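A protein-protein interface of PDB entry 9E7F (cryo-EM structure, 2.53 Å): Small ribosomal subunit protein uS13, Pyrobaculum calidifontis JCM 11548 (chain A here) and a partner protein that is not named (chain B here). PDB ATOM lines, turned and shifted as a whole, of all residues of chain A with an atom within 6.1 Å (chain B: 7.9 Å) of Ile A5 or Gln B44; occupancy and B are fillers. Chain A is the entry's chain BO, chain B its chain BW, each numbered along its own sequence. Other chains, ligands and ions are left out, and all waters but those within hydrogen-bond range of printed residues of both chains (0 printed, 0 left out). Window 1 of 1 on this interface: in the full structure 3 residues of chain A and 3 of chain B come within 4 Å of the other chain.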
ATOM      1  N   ALA A   2      14.588 -15.426  -8.032  1.00  0.00           N
ATOM      2  CA  ALA A   2      14.147 -14.586  -9.137  1.00  0.00           C
ATOM      3  C   ALA A   2      12.849 -13.864  -8.794  1.00  0.00           C
ATOM      4  O   ALA A   2      12.513 -13.696  -7.624  1.00  0.00           O
ATOM      5  CB  ALA A   2      13.975 -15.417 -10.402  1.00  0.00           C
ATOM      6  N   GLN A   3      12.123 -13.433  -9.824  1.00  0.00           N
ATOM      7  CA  GLN A   3      10.884 -12.691  -9.625  1.00  0.00           C
ATOM      8  C   GLN A   3       9.712 -13.665  -9.574  1.00  0.00           C
ATOM      9  O   GLN A   3       9.512 -14.454 -10.502  1.00  0.00           O
ATOM     10  CB  GLN A   3      10.696 -11.665 -10.739  1.00  0.00           C
ATOM     11  CG  GLN A   3       9.710 -10.550 -10.415  1.00  0.00           C
ATOM     12  CD  GLN A   3       8.276 -10.914 -10.745  1.00  0.00           C
ATOM     13  OE1 GLN A   3       8.019 -11.843 -11.509  1.00  0.00           O
ATOM     14  NE2 GLN A   3       7.332 -10.172 -10.178  1.00  0.00           N
ATOM     15  N   GLU A   4       8.944 -13.608  -8.489  1.00  0.00           N
ATOM     16  CA  GLU A   4       7.807 -14.501  -8.312  1.00  0.00           C
ATOM     17  C   GLU A   4       6.731 -14.205  -9.345  1.00  0.00           C
ATOM     18  O   GLU A   4       6.454 -13.041  -9.645  1.00  0.00           O
ATOM     19  CB  GLU A   4       7.251 -14.352  -6.899  1.00  0.00           C
ATOM     20  CG  GLU A   4       6.844 -15.659  -6.239  1.00  0.00           C
ATOM     21  CD  GLU A   4       8.026 -16.556  -5.909  1.00  0.00           C
ATOM     22  OE1 GLU A   4       9.172 -16.210  -6.275  1.00  0.00           O
ATOM     23  OE2 GLU A   4       7.808 -17.608  -5.270  1.00  0.00           O
ATOM     24  N   ILE A   5       6.121 -15.266  -9.877  1.00  0.00           N
ATOM     25  CA  ILE A   5       5.179 -15.129 -10.980  1.00  0.00           C
ATOM     26  C   ILE A   5       3.951 -14.363 -10.525  1.00  0.00           C
ATOM     27  O   ILE A   5       3.293 -14.734  -9.549  1.00  0.00           O
ATOM     28  CB  ILE A   5       4.801 -16.517 -11.523  1.00  0.00           C
ATOM     29  CG1 ILE A   5       6.036 -17.228 -12.072  1.00  0.00           C
ATOM     30  CG2 ILE A   5       3.726 -16.401 -12.585  1.00  0.00           C
ATOM     31  CD1 ILE A   5       6.467 -18.417 -11.248  1.00  0.00           C
ATOM     32  N   ARG A   6       3.644 -13.281 -11.232  1.00  0.00           N
ATOM     33  CA  ARG A   6       2.460 -12.486 -10.931  1.00  0.00           C
ATOM     34  C   ARG A   6       1.216 -13.304 -11.232  1.00  0.00           C
ATOM     35  O   ARG A   6       0.964 -13.648 -12.388  1.00  0.00           O
ATOM     36  CB  ARG A   6       2.455 -11.206 -11.753  1.00  0.00           C
ATOM     37  CG  ARG A   6       3.733 -10.412 -11.752  1.00  0.00           C
ATOM     38  CD  ARG A   6       3.660  -9.050 -12.486  1.00  0.00           C
ATOM     39  NE  ARG A   6       2.635  -8.108 -12.029  1.00  0.00           N
ATOM     40  CZ  ARG A   6       1.327  -8.175 -12.256  1.00  0.00           C
ATOM     41  NH1 ARG A   6       0.812  -9.006 -13.143  1.00  0.00           N
ATOM     42  NH2 ARG A   6       0.518  -7.333 -11.621  1.00  0.00           N
ATOM     43  N   ALA A   7       0.427 -13.604 -10.201  1.00  0.00           N
ATOM     44  CA  ALA A   7      -0.768 -14.416 -10.404  1.00  0.00           C
ATOM     45  C   ALA A   7      -1.804 -13.684 -11.248  1.00  0.00           C
ATOM     46  O   ALA A   7      -2.543 -14.309 -12.017  1.00  0.00           O
ATOM     47  CB  ALA A   7      -1.363 -14.823  -9.058  1.00  0.00           C
ATOM     48  N   ILE A   8      -1.875 -12.364 -11.121  1.00  0.00           N
ATOM     49  CA  ILE A   8      -2.880 -11.559 -11.800  1.00  0.00           C
ATOM     50  C   ILE A   8      -2.198 -10.543 -12.703  1.00  0.00           C
ATOM     51  O   ILE A   8      -1.280  -9.834 -12.276  1.00  0.00           O
ATOM     52  CB  ILE A   8      -3.805 -10.848 -10.794  1.00  0.00           C
ATOM     53  CG1 ILE A   8      -4.766 -11.848 -10.152  1.00  0.00           C
ATOM     54  CG2 ILE A   8      -4.527  -9.707 -11.461  1.00  0.00           C
ATOM     55  CD1 ILE A   8      -5.098 -13.025 -11.029  1.00  0.00           C
ATOM     56  N   GLY A  18      -1.545 -15.035 -14.657  1.00  0.00           N
ATOM     57  CA  GLY A  18      -0.115 -14.928 -14.859  1.00  0.00           C
ATOM     58  C   GLY A  18       0.597 -16.252 -14.992  1.00  0.00           C
ATOM     59  O   GLY A  18       1.744 -16.281 -15.448  1.00  0.00           O
ATOM     60  N   ASN A  19      -0.056 -17.348 -14.613  1.00  0.00           N
ATOM     61  CA  ASN A  19       0.514 -18.677 -14.748  1.00  0.00           C
ATOM     62  C   ASN A  19       0.174 -19.326 -16.083  1.00  0.00           C
ATOM     63  O   ASN A  19       0.585 -20.462 -16.330  1.00  0.00           O
ATOM     64  CB  ASN A  19       0.052 -19.567 -13.599  1.00  0.00           C
ATOM     65  CG  ASN A  19       1.080 -19.666 -12.493  1.00  0.00           C
ATOM     66  OD1 ASN A  19       2.089 -20.357 -12.628  1.00  0.00           O
ATOM     67  ND2 ASN A  19       0.828 -18.976 -11.389  1.00  0.00           N
ATOM     68  N   THR A  51       5.778 -17.240 -20.347  1.00  0.00           N
ATOM     69  CA  THR A  51       4.858 -17.040 -19.239  1.00  0.00           C
ATOM     70  C   THR A  51       4.502 -15.566 -19.142  1.00  0.00           C
ATOM     71  O   THR A  51       5.385 -14.713 -19.025  1.00  0.00           O
ATOM     72  CB  THR A  51       5.469 -17.530 -17.937  1.00  0.00           C
ATOM     73  OG1 THR A  51       5.985 -18.851 -18.127  1.00  0.00           O
ATOM     74  CG2 THR A  51       4.411 -17.571 -16.865  1.00  0.00           C
ATOM     75  N   GLY A  53       3.110 -13.973 -16.785  1.00  0.00           N
ATOM     76  CA  GLY A  53       3.420 -13.393 -15.490  1.00  0.00           C
ATOM     77  C   GLY A  53       4.810 -12.796 -15.410  1.00  0.00           C
ATOM     78  O   GLY A  53       5.002 -11.746 -14.797  1.00  0.00           O
ATOM     79  N   LEU A  54       5.790 -13.437 -16.036  1.00  0.00           N
ATOM     80  CA  LEU A  54       7.179 -13.009 -15.953  1.00  0.00           C
ATOM     81  C   LEU A  54       7.563 -12.002 -17.027  1.00  0.00           C
ATOM     82  O   LEU A  54       8.730 -11.607 -17.089  1.00  0.00           O
ATOM     83  CB  LEU A  54       8.106 -14.221 -16.041  1.00  0.00           C
ATOM     84  CG  LEU A  54       7.682 -15.445 -15.231  1.00  0.00           C
ATOM     85  CD1 LEU A  54       8.175 -16.712 -15.895  1.00  0.00           C
ATOM     86  CD2 LEU A  54       8.199 -15.356 -13.812  1.00  0.00           C
ATOM     87  N   ARG B  41      17.255 -20.479  -9.338  1.00  0.00           N
ATOM     88  CA  ARG B  41      15.904 -20.794  -9.788  1.00  0.00           C
ATOM     89  C   ARG B  41      15.907 -21.320 -11.222  1.00  0.00           C
ATOM     90  O   ARG B  41      15.472 -20.631 -12.144  1.00  0.00           O
ATOM     91  CB  ARG B  41      15.003 -19.558  -9.673  1.00  0.00           C
ATOM     92  CG  ARG B  41      13.536 -19.807 -10.002  1.00  0.00           C
ATOM     93  CD  ARG B  41      12.646 -19.660  -8.793  1.00  0.00           C
ATOM     94  NE  ARG B  41      11.239 -19.571  -9.165  1.00  0.00           N
ATOM     95  CZ  ARG B  41      10.281 -19.117  -8.370  1.00  0.00           C
ATOM     96  NH1 ARG B  41      10.542 -18.697  -7.145  1.00  0.00           N
ATOM     97  NH2 ARG B  41       9.029 -19.088  -8.815  1.00  0.00           N
ATOM     98  N   THR B  42      16.425 -22.532 -11.414  1.00  0.00           N
ATOM     99  CA  THR B  42      16.250 -23.209 -12.689  1.00  0.00           C
ATOM    100  C   THR B  42      14.810 -23.679 -12.823  1.00  0.00           C
ATOM    101  O   THR B  42      14.165 -24.038 -11.837  1.00  0.00           O
ATOM    102  CB  THR B  42      17.200 -24.398 -12.822  1.00  0.00           C
ATOM    103  OG1 THR B  42      16.772 -25.225 -13.909  1.00  0.00           O
ATOM    104  CG2 THR B  42      17.202 -25.223 -11.568  1.00  0.00           C
ATOM    105  N   ILE B  43      14.314 -23.683 -14.063  1.00  0.00           N
ATOM    106  CA  ILE B  43      12.883 -23.771 -14.337  1.00  0.00           C
ATOM    107  C   ILE B  43      12.220 -22.575 -13.675  1.00  0.00           C
ATOM    108  O   ILE B  43      11.980 -22.576 -12.463  1.00  0.00           O
ATOM    109  CB  ILE B  43      12.263 -25.095 -13.857  1.00  0.00           C
ATOM    110  CG1 ILE B  43      13.201 -26.268 -14.140  1.00  0.00           C
ATOM    111  CG2 ILE B  43      10.912 -25.310 -14.494  1.00  0.00           C
ATOM    112  CD1 ILE B  43      13.215 -26.709 -15.571  1.00  0.00           C
ATOM    113  N   GLN B  44      11.933 -21.545 -14.472  1.00  0.00           N
ATOM    114  CA  GLN B  44      11.506 -20.233 -14.001  1.00  0.00           C
ATOM    115  C   GLN B  44      10.259 -20.270 -13.129  1.00  0.00           C
ATOM    116  O   GLN B  44      10.127 -19.475 -12.194  1.00  0.00           O
ATOM    117  CB  GLN B  44      11.252 -19.320 -15.199  1.00  0.00           C
ATOM    118  CG  GLN B  44      12.504 -18.754 -15.828  1.00  0.00           C
ATOM    119  CD  GLN B  44      12.391 -17.264 -16.058  1.00  0.00           C
ATOM    120  OE1 GLN B  44      11.419 -16.791 -16.643  1.00  0.00           O
ATOM    121  NE2 GLN B  44      13.379 -16.514 -15.588  1.00  0.00           N
ATOM    122  N   THR B  45       9.343 -21.187 -13.422  1.00  0.00           N
ATOM    123  CA  THR B  45       8.064 -21.191 -12.732  1.00  0.00           C
ATOM    124  C   THR B  45       8.122 -21.878 -11.375  1.00  0.00           C
ATOM    125  O   THR B  45       7.172 -21.756 -10.598  1.00  0.00           O
ATOM    126  CB  THR B  45       7.005 -21.866 -13.597  1.00  0.00           C
ATOM    127  OG1 THR B  45       6.999 -23.272 -13.326  1.00  0.00           O
ATOM    128  CG2 THR B  45       7.303 -21.635 -15.073  1.00  0.00           C
ATOM    129  N   LEU B  46       9.201 -22.588 -11.073  1.00  0.00           N
ATOM    130  CA  LEU B  46       9.318 -23.349  -9.842  1.00  0.00           C
ATOM    131  C   LEU B  46      10.443 -22.784  -8.990  1.00  0.00           C
ATOM    132  O   LEU B  46      11.524 -22.478  -9.499  1.00  0.00           O
ATOM    133  CB  LEU B  46       9.587 -24.824 -10.138  1.00  0.00           C
ATOM    134  CG  LEU B  46       9.550 -25.764  -8.940  1.00  0.00           C
ATOM    135  CD1 LEU B  46       8.179 -25.702  -8.312  1.00  0.00           C
ATOM    136  CD2 LEU B  46       9.891 -27.178  -9.352  1.00  0.00           C
ATOM    137  N   ASP B  47      10.177 -22.667  -7.689  1.00  0.00           N
ATOM    138  CA  ASP B  47      11.191 -22.108  -6.759  1.00  0.00           C
ATOM    139  C   ASP B  47      12.294 -23.138  -6.520  1.00  0.00           C
ATOM    140  O   ASP B  47      12.016 -24.349  -6.631  1.00  0.00           O
ATOM    141  CB  ASP B  47      10.552 -21.676  -5.440  1.00  0.00           C
ATOM    142  CG  ASP B  47       9.949 -22.840  -4.675  1.00  0.00           C
ATOM    143  OD1 ASP B  47       8.734 -23.067  -4.823  1.00  0.00           O
ATOM    144  OD2 ASP B  47      10.702 -23.509  -3.946  1.00  0.00           O
ATOM    145  N   GLU B  48      13.491 -22.665  -6.179  1.00  0.00           N
ATOM    146  CA  GLU B  48      14.617 -23.558  -5.930  1.00  0.00           C
ATOM    147  C   GLU B  48      14.424 -24.387  -4.669  1.00  0.00           C
ATOM    148  O   GLU B  48      15.045 -25.445  -4.524  1.00  0.00           O
ATOM    149  CB  GLU B  48      15.915 -22.769  -5.826  1.00  0.00           C
ATOM    150  CG  GLU B  48      16.681 -22.698  -7.118  1.00  0.00           C
ATOM    151  CD  GLU B  48      16.715 -24.021  -7.832  1.00  0.00           C
ATOM    152  OE1 GLU B  48      17.150 -25.020  -7.220  1.00  0.00           O
ATOM    153  OE2 GLU B  48      16.302 -24.053  -9.005  1.00  0.00           O
ATOM    154  N   LEU B  79       4.390 -28.948 -15.489  1.00  0.00           N
ATOM    155  CA  LEU B  79       5.527 -28.433 -14.733  1.00  0.00           C
ATOM    156  C   LEU B  79       6.398 -29.570 -14.222  1.00  0.00           C
ATOM    157  O   LEU B  79       7.619 -29.424 -14.115  1.00  0.00           O
ATOM    158  CB  LEU B  79       5.035 -27.559 -13.580  1.00  0.00           C
ATOM    159  CG  LEU B  79       6.065 -26.863 -12.687  1.00  0.00           C
ATOM    160  CD1 LEU B  79       6.445 -27.718 -11.485  1.00  0.00           C
ATOM    161  CD2 LEU B  79       7.297 -26.463 -13.483  1.00  0.00           C
ATOM    162  N   LYS B  82       9.229 -30.651 -17.102  1.00  0.00           N
ATOM    163  CA  LYS B  82      10.483 -29.928 -17.286  1.00  0.00           C
ATOM    164  C   LYS B  82      11.416 -30.121 -16.103  1.00  0.00           C
ATOM    165  O   LYS B  82      12.630 -29.940 -16.238  1.00  0.00           O
ATOM    166  CB  LYS B  82      10.232 -28.438 -17.513  1.00  0.00           C
ATOM    167  CG  LYS B  82       8.968 -28.106 -18.258  1.00  0.00           C
ATOM    168  CD  LYS B  82       8.737 -26.610 -18.246  1.00  0.00           C
ATOM    169  CE  LYS B  82       7.302 -26.268 -18.586  1.00  0.00           C
ATOM    170  NZ  LYS B  82       6.338 -27.008 -17.728  1.00  0.00           N
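Arg B41 touches Ile A5. O of Gln B44 touches CD1 of Ile A5 (3.9 Å). CD1 of Ile A5 touches O of Thr B45, at 3.5 Å. Leu A54 touches Gln B44 (CD1 to OE1, 3.3 Å).
Gln B44 touches just these residues of chain A: Ile A5 (3.9 Å) and Leu A54 (3.3 Å). Printed residues of chain B within 4 Å of Leu A54: Gln B44 (3.3 Å). Of the printed residues of chain A, Arg B41 touches Glu A4 (3.0 Å) and Ile A5 (3.6 Å). Printed residues of chain A within 4 Å of Thr B45: Ile A5. Printed residues of chain B within 4 Å of Glu A4: Arg B41. Asn A19 touches none of the printed residues of chain B. The nearest printed residue of chain A that does not touch Arg B41 is Ala A2 (4.3 Å).
NE of Arg B41 lies within hydrogen-bond range of O of Gln B44, at 3.2 Å. The guanidinium group of Arg B41 is in hydrogen-bond range of the backbone carbonyl oxygen of Leu B46, at 2.9 Å.
Of the 12 printed residues of chain A, 3 touch a printed residue of chain B. Hydrophobic or aromatic side chains of chain A that line the printed part of chain B: Ile A5 and Leu A54. Along chain B the printed residues that touch a printed residue of chain A span positions 41 to 45. Among the printed residues, Asp or Glu carboxylates within 4 Å of a Lys or Arg side-chain nitrogen of the other chain: Glu A4 with Arg B41.
OE1 of Glu A4 lies within salt-bridge range of NH1 of Arg B41 (3.0 Å).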
